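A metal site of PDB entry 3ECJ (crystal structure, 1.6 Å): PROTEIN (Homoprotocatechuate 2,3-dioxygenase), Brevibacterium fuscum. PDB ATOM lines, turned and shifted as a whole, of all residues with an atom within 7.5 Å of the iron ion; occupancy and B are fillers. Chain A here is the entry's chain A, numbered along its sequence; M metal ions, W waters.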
ATOM      1  N   ASP A 154      34.545  19.086   2.632  1.00  0.00           N
ATOM      2  CA  ASP A 154      33.253  19.762   2.660  1.00  0.00           C
ATOM      3  C   ASP A 154      32.115  18.949   3.229  1.00  0.00           C
ATOM      4  O   ASP A 154      31.351  19.465   4.046  1.00  0.00           O
ATOM      5  CB  ASP A 154      32.833  20.319   1.293  1.00  0.00           C
ATOM      6  CG  ASP A 154      31.592  21.205   1.395  1.00  0.00           C
ATOM      7  OD1 ASP A 154      31.745  22.390   1.830  1.00  0.00           O
ATOM      8  OD2 ASP A 154      30.463  20.724   1.115  1.00  0.00           O
ATOM      9  N   HIS A 155      31.979  17.699   2.805  1.00  0.00           N
ATOM     10  CA  HIS A 155      30.845  16.890   3.286  1.00  0.00           C
ATOM     11  C   HIS A 155      30.969  15.402   3.061  1.00  0.00           C
ATOM     12  O   HIS A 155      31.858  14.938   2.363  1.00  0.00           O
ATOM     13  CB  HIS A 155      29.532  17.406   2.649  1.00  0.00           C
ATOM     14  CG  HIS A 155      29.440  17.193   1.162  1.00  0.00           C
ATOM     15  ND1 HIS A 155      29.765  18.178   0.246  1.00  0.00           N
ATOM     16  CD2 HIS A 155      29.009  16.131   0.441  1.00  0.00           C
ATOM     17  CE1 HIS A 155      29.536  17.731  -0.977  1.00  0.00           C
ATOM     18  NE2 HIS A 155      29.083  16.491  -0.883  1.00  0.00           N
ATOM     19  N   PHE A 156      30.056  14.649   3.695  1.00  0.00           N
ATOM     20  CA  PHE A 156      29.854  13.248   3.396  1.00  0.00           C
ATOM     21  C   PHE A 156      28.481  13.100   2.702  1.00  0.00           C
ATOM     22  O   PHE A 156      27.624  13.985   2.799  1.00  0.00           O
ATOM     23  CB  PHE A 156      29.801  12.394   4.671  1.00  0.00           C
ATOM     24  CG  PHE A 156      30.949  12.623   5.635  1.00  0.00           C
ATOM     25  CD1 PHE A 156      32.273  12.419   5.244  1.00  0.00           C
ATOM     26  CD2 PHE A 156      30.702  13.033   6.938  1.00  0.00           C
ATOM     27  CE1 PHE A 156      33.332  12.622   6.173  1.00  0.00           C
ATOM     28  CE2 PHE A 156      31.747  13.218   7.866  1.00  0.00           C
ATOM     29  CZ  PHE A 156      33.054  13.039   7.474  1.00  0.00           C
ATOM     30  N   ASN A 157      28.293  11.977   2.029  1.00  0.00           N
ATOM     31  CA  ASN A 157      26.970  11.648   1.509  1.00  0.00           C
ATOM     32  C   ASN A 157      26.700  10.157   1.745  1.00  0.00           C
ATOM     33  O   ASN A 157      27.495   9.322   1.361  1.00  0.00           O
ATOM     34  CB  ASN A 157      26.880  11.998   0.019  1.00  0.00           C
ATOM     35  CG  ASN A 157      25.481  11.884  -0.518  1.00  0.00           C
ATOM     36  OD1 ASN A 157      24.886  10.813  -0.432  1.00  0.00           O
ATOM     37  ND2 ASN A 157      24.945  12.975  -1.070  1.00  0.00           N
ATOM     38  N   TRP A 192      19.635  17.178   2.080  1.00  0.00           N
ATOM     39  CA  TRP A 192      20.953  17.765   2.400  1.00  0.00           C
ATOM     40  C   TRP A 192      20.827  18.513   3.714  1.00  0.00           C
ATOM     41  O   TRP A 192      19.850  19.256   3.914  1.00  0.00           O
ATOM     42  CB  TRP A 192      21.344  18.776   1.305  1.00  0.00           C
ATOM     43  CG  TRP A 192      21.809  18.160   0.023  1.00  0.00           C
ATOM     44  CD1 TRP A 192      23.101  18.107  -0.440  1.00  0.00           C
ATOM     45  CD2 TRP A 192      21.003  17.508  -0.971  1.00  0.00           C
ATOM     46  NE1 TRP A 192      23.157  17.448  -1.649  1.00  0.00           N
ATOM     47  CE2 TRP A 192      21.878  17.075  -1.999  1.00  0.00           C
ATOM     48  CE3 TRP A 192      19.626  17.247  -1.112  1.00  0.00           C
ATOM     49  CZ2 TRP A 192      21.435  16.402  -3.143  1.00  0.00           C
ATOM     50  CZ3 TRP A 192      19.190  16.563  -2.250  1.00  0.00           C
ATOM     51  CH2 TRP A 192      20.085  16.142  -3.242  1.00  0.00           C
ATOM     52  N   HIS A 200      25.747  21.681   3.113  1.00  0.00           N
ATOM     53  CA  HIS A 200      25.727  20.470   3.934  1.00  0.00           C
ATOM     54  C   HIS A 200      27.056  20.028   4.536  1.00  0.00           C
ATOM     55  O   HIS A 200      28.129  20.383   4.063  1.00  0.00           O
ATOM     56  CB  HIS A 200      25.075  19.286   3.220  1.00  0.00           C
ATOM     57  CG  HIS A 200      25.723  18.884   1.928  1.00  0.00           C
ATOM     58  ND1 HIS A 200      26.111  19.791   0.956  1.00  0.00           N
ATOM     59  CD2 HIS A 200      25.937  17.656   1.405  1.00  0.00           C
ATOM     60  CE1 HIS A 200      26.574  19.131  -0.096  1.00  0.00           C
ATOM     61  NE2 HIS A 200      26.474  17.831   0.152  1.00  0.00           N
ATOM     62  N   ALA A 203      24.566  14.241   3.933  1.00  0.00           N
ATOM     63  CA  ALA A 203      23.382  14.209   3.090  1.00  0.00           C
ATOM     64  C   ALA A 203      22.921  12.774   3.013  1.00  0.00           C
ATOM     65  O   ALA A 203      23.700  11.842   3.195  1.00  0.00           O
ATOM     66  CB  ALA A 203      23.706  14.714   1.697  1.00  0.00           C
ATOM     67  N   THR A 205      21.055  10.030   0.542  1.00  0.00           N
ATOM     68  CA  THR A 205      20.640   9.631  -0.794  1.00  0.00           C
ATOM     69  C   THR A 205      19.840   8.334  -0.678  1.00  0.00           C
ATOM     70  O   THR A 205      20.299   7.376  -0.068  1.00  0.00           O
ATOM     71  CB  THR A 205      21.861   9.413  -1.721  1.00  0.00           C
ATOM     72  OG1 THR A 205      22.599  10.645  -1.820  1.00  0.00           O
ATOM     73  CG2 THR A 205      21.426   8.956  -3.115  1.00  0.00           C
ATOM     74  N   HIS A 213      28.017   7.027  -0.010  1.00  0.00           N
ATOM     75  CA  HIS A 213      27.978   7.415  -1.394  1.00  0.00           C
ATOM     76  C   HIS A 213      29.298   8.076  -1.803  1.00  0.00           C
ATOM     77  O   HIS A 213      29.899   7.664  -2.793  1.00  0.00           O
ATOM     78  CB  HIS A 213      26.788   8.328  -1.729  1.00  0.00           C
ATOM     79  CG  HIS A 213      26.502   8.377  -3.190  1.00  0.00           C
ATOM     80  ND1 HIS A 213      27.220   9.181  -4.049  1.00  0.00           N
ATOM     81  CD2 HIS A 213      25.637   7.675  -3.952  1.00  0.00           C
ATOM     82  CE1 HIS A 213      26.786   8.982  -5.279  1.00  0.00           C
ATOM     83  NE2 HIS A 213      25.810   8.087  -5.254  1.00  0.00           N
ATOM     84  N   HIS A 214      29.709   9.106  -1.048  1.00  0.00           N
ATOM     85  CA  HIS A 214      30.983   9.800  -1.329  1.00  0.00           C
ATOM     86  C   HIS A 214      31.476  10.661  -0.173  1.00  0.00           C
ATOM     87  O   HIS A 214      30.733  10.945   0.788  1.00  0.00           O
ATOM     88  CB  HIS A 214      30.870  10.660  -2.621  1.00  0.00           C
ATOM     89  CG  HIS A 214      29.799  11.715  -2.568  1.00  0.00           C
ATOM     90  ND1 HIS A 214      28.531  11.502  -3.066  1.00  0.00           N
ATOM     91  CD2 HIS A 214      29.834  13.023  -2.196  1.00  0.00           C
ATOM     92  CE1 HIS A 214      27.815  12.617  -2.945  1.00  0.00           C
ATOM     93  NE2 HIS A 214      28.577  13.553  -2.423  1.00  0.00           N
ATOM     94  N   VAL A 215      32.746  11.085  -0.266  1.00  0.00           N
ATOM     95  CA  VAL A 215      33.327  12.111   0.584  1.00  0.00           C
ATOM     96  C   VAL A 215      33.653  13.250  -0.405  1.00  0.00           C
ATOM     97  O   VAL A 215      34.126  12.947  -1.491  1.00  0.00           O
ATOM     98  CB  VAL A 215      34.648  11.607   1.232  1.00  0.00           C
ATOM     99  CG1 VAL A 215      35.315  12.704   2.006  1.00  0.00           C
ATOM    100  CG2 VAL A 215      34.348  10.443   2.171  1.00  0.00           C
ATOM    101  N   ALA A 216      33.393  14.506  -0.026  1.00  0.00           N
ATOM    102  CA  ALA A 216      33.597  15.648  -0.927  1.00  0.00           C
ATOM    103  C   ALA A 216      34.658  16.587  -0.386  1.00  0.00           C
ATOM    104  O   ALA A 216      34.625  16.945   0.799  1.00  0.00           O
ATOM    105  CB  ALA A 216      32.288  16.429  -1.107  1.00  0.00           C
ATOM    106  N   HIS A 248      25.726  21.736 -10.142  1.00  0.00           N
ATOM    107  CA  HIS A 248      24.605  21.095  -9.459  1.00  0.00           C
ATOM    108  C   HIS A 248      23.400  22.013  -9.484  1.00  0.00           C
ATOM    109  O   HIS A 248      23.540  23.251  -9.427  1.00  0.00           O
ATOM    110  CB  HIS A 248      24.927  20.841  -7.987  1.00  0.00           C
ATOM    111  CG  HIS A 248      25.725  19.596  -7.717  1.00  0.00           C
ATOM    112  ND1 HIS A 248      25.410  18.370  -8.255  1.00  0.00           N
ATOM    113  CD2 HIS A 248      26.795  19.399  -6.910  1.00  0.00           C
ATOM    114  CE1 HIS A 248      26.274  17.472  -7.810  1.00  0.00           C
ATOM    115  NE2 HIS A 248      27.110  18.058  -6.974  1.00  0.00           N
ATOM    116  N   SER A 251      22.262  22.671  -4.300  1.00  0.00           N
ATOM    117  CA  SER A 251      23.553  23.178  -3.760  1.00  0.00           C
ATOM    118  C   SER A 251      24.158  24.299  -4.633  1.00  0.00           C
ATOM    119  O   SER A 251      24.898  25.128  -4.102  1.00  0.00           O
ATOM    120  CB  SER A 251      24.600  22.090  -3.496  1.00  0.00           C
ATOM    121  OG  SER A 251      25.272  21.718  -4.701  1.00  0.00           O
ATOM    122  N   TYR A 255      30.985  20.806  -9.688  1.00  0.00           N
ATOM    123  CA  TYR A 255      31.266  19.478  -9.122  1.00  0.00           C
ATOM    124  C   TYR A 255      31.925  18.513 -10.090  1.00  0.00           C
ATOM    125  O   TYR A 255      31.856  18.704 -11.324  1.00  0.00           O
ATOM    126  CB  TYR A 255      29.974  18.838  -8.610  1.00  0.00           C
ATOM    127  CG  TYR A 255      29.074  18.338  -9.710  1.00  0.00           C
ATOM    128  CD1 TYR A 255      28.021  19.129 -10.195  1.00  0.00           C
ATOM    129  CD2 TYR A 255      29.281  17.082 -10.283  1.00  0.00           C
ATOM    130  CE1 TYR A 255      27.176  18.657 -11.229  1.00  0.00           C
ATOM    131  CE2 TYR A 255      28.454  16.607 -11.309  1.00  0.00           C
ATOM    132  CZ  TYR A 255      27.404  17.401 -11.772  1.00  0.00           C
ATOM    133  OH  TYR A 255      26.590  16.916 -12.780  1.00  0.00           O
ATOM    134  N   TYR A 257      32.740  13.930  -9.963  1.00  0.00           N
ATOM    135  CA  TYR A 257      32.836  12.668  -9.208  1.00  0.00           C
ATOM    136  C   TYR A 257      33.863  11.753  -9.849  1.00  0.00           C
ATOM    137  O   TYR A 257      33.777  11.495 -11.048  1.00  0.00           O
ATOM    138  CB  TYR A 257      31.495  11.924  -9.134  1.00  0.00           C
ATOM    139  CG  TYR A 257      30.389  12.707  -8.465  1.00  0.00           C
ATOM    140  CD1 TYR A 257      30.230  12.693  -7.075  1.00  0.00           C
ATOM    141  CD2 TYR A 257      29.536  13.529  -9.214  1.00  0.00           C
ATOM    142  CE1 TYR A 257      29.210  13.466  -6.461  1.00  0.00           C
ATOM    143  CE2 TYR A 257      28.526  14.261  -8.640  1.00  0.00           C
ATOM    144  CZ  TYR A 257      28.360  14.246  -7.263  1.00  0.00           C
ATOM    145  OH  TYR A 257      27.352  14.995  -6.715  1.00  0.00           O
ATOM    146  N   GLU A 267      33.945  13.324  -4.420  1.00  0.00           N
ATOM    147  CA  GLU A 267      33.427  14.472  -5.155  1.00  0.00           C
ATOM    148  C   GLU A 267      34.353  15.651  -4.933  1.00  0.00           C
ATOM    149  O   GLU A 267      34.855  15.845  -3.819  1.00  0.00           O
ATOM    150  CB  GLU A 267      32.019  14.866  -4.691  1.00  0.00           C
ATOM    151  CG  GLU A 267      31.380  16.006  -5.533  1.00  0.00           C
ATOM    152  CD  GLU A 267      30.046  16.453  -4.957  1.00  0.00           C
ATOM    153  OE1 GLU A 267      29.669  15.877  -3.926  1.00  0.00           O
ATOM    154  OE2 GLU A 267      29.385  17.340  -5.534  1.00  0.00           O
ATOM    155  N   ILE A 268      34.591  16.434  -5.991  1.00  0.00           N
ATOM    156  CA  ILE A 268      35.253  17.721  -5.881  1.00  0.00           C
ATOM    157  C   ILE A 268      34.169  18.781  -6.118  1.00  0.00           C
ATOM    158  O   ILE A 268      33.339  18.631  -7.022  1.00  0.00           O
ATOM    159  CB  ILE A 268      36.377  17.906  -6.904  1.00  0.00           C
ATOM    160  CG1 ILE A 268      37.139  16.592  -7.143  1.00  0.00           C
ATOM    161  CG2 ILE A 268      37.290  19.015  -6.438  1.00  0.00           C
ATOM    162  CD1 ILE A 268      37.882  16.057  -5.917  1.00  0.00           C
ATOM    163  N   TYR A 269      34.190  19.869  -5.343  1.00  0.00           N
ATOM    164  CA  TYR A 269      33.006  20.701  -5.109  1.00  0.00           C
ATOM    165  C   TYR A 269      33.488  22.127  -4.869  1.00  0.00           C
ATOM    166  O   TYR A 269      34.522  22.339  -4.226  1.00  0.00           O
ATOM    167  CB  TYR A 269      32.329  20.124  -3.846  1.00  0.00           C
ATOM    168  CG  TYR A 269      31.053  20.725  -3.322  1.00  0.00           C
ATOM    169  CD1 TYR A 269      29.815  20.166  -3.664  1.00  0.00           C
ATOM    170  CD2 TYR A 269      31.068  21.751  -2.369  1.00  0.00           C
ATOM    171  CE1 TYR A 269      28.632  20.660  -3.145  1.00  0.00           C
ATOM    172  CE2 TYR A 269      29.887  22.249  -1.828  1.00  0.00           C
ATOM    173  CZ  TYR A 269      28.673  21.695  -2.229  1.00  0.00           C
ATOM    174  OH  TYR A 269      27.491  22.170  -1.693  1.00  0.00           O
ATOM    175  N   TRP A 304      26.085   6.126 -10.628  1.00  0.00           N
ATOM    176  CA  TRP A 304      25.954   7.093  -9.559  1.00  0.00           C
ATOM    177  C   TRP A 304      24.798   6.702  -8.626  1.00  0.00           C
ATOM    178  O   TRP A 304      24.862   6.908  -7.398  1.00  0.00           O
ATOM    179  CB  TRP A 304      25.793   8.527 -10.132  1.00  0.00           C
ATOM    180  CG  TRP A 304      26.120   9.608  -9.147  1.00  0.00           C
ATOM    181  CD1 TRP A 304      27.339  10.215  -8.977  1.00  0.00           C
ATOM    182  CD2 TRP A 304      25.231  10.208  -8.200  1.00  0.00           C
ATOM    183  NE1 TRP A 304      27.268  11.147  -7.965  1.00  0.00           N
ATOM    184  CE2 TRP A 304      25.986  11.179  -7.482  1.00  0.00           C
ATOM    185  CE3 TRP A 304      23.875  10.022  -7.872  1.00  0.00           C
ATOM    186  CZ2 TRP A 304      25.434  11.950  -6.458  1.00  0.00           C
ATOM    187  CZ3 TRP A 304      23.320  10.795  -6.839  1.00  0.00           C
ATOM    188  CH2 TRP A 304      24.106  11.754  -6.150  1.00  0.00           C
HETATM  189 FE    FE M   1      28.032  15.652  -2.650  1.00  0.00          FE
HETATM  190  O   HOH W   1      26.594  14.967  -4.256  1.00  0.00           O
HETATM  191  O   HOH W   2      26.212  15.440  -1.563  1.00  0.00           O
HETATM  192  O   HOH W   3      27.485  17.692  -3.463  1.00  0.00           O
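The backbone NH (N) of Glu 267 sits at hydrogen-bond distance from the backbone carbonyl oxygen (O) of Val 215 (3.0 Å).
The side-chain carboxylate (OE2) of Glu 267 lies within hydrogen-bond range of the side-chain hydroxyl (OH) of Tyr 257 (3.3 Å).
A ring nitrogen (ND1) of His 155 sits at hydrogen-bond distance from the side-chain carboxylate (OD2) of Asp 154, 2.8 Å away.
The backbone carbonyl oxygen of His 214 sits at hydrogen-bond distance from the backbone NH of Asn 157.
The backbone NH (N) of Ala 216 is in hydrogen-bond range of the backbone carbonyl oxygen (O) of His 155 (2.9 Å).
A ring nitrogen (ND1) of His 155 lies close to a ring nitrogen (NE2) of His 200 (3.3 Å).
A ring nitrogen (ND1) of His 214 lies within hydrogen-bond range of a ring nitrogen (ND1) of His 213.
NE2 of His 248 lies within hydrogen-bond range of OE2 of Glu 267 (2.8 Å).
Residues that only touch the iron ion: His 200.
Within 4 Å of the iron ion: His 155, His 200, His 214 and Glu 267.
The nearest printed residue that does not touch the iron ion is Tyr 257 (4.2 Å).
The iron ion is bound by the side-chain carboxylate (OE1) of Glu 267 (2.1 Å), water W2 (2.1 Å), a ring nitrogen (NE2) of His 214 (2.2 Å), a ring nitrogen (NE2) of His 155 (2.2 Å), water W1 (2.3 Å) and water W3 (2.3 Å).
The iron ion has six donor atoms within binding distance.
Water W2 bridges the side-chain amide nitrogen of Asn 157 and a ring nitrogen (NE2) of His 200.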
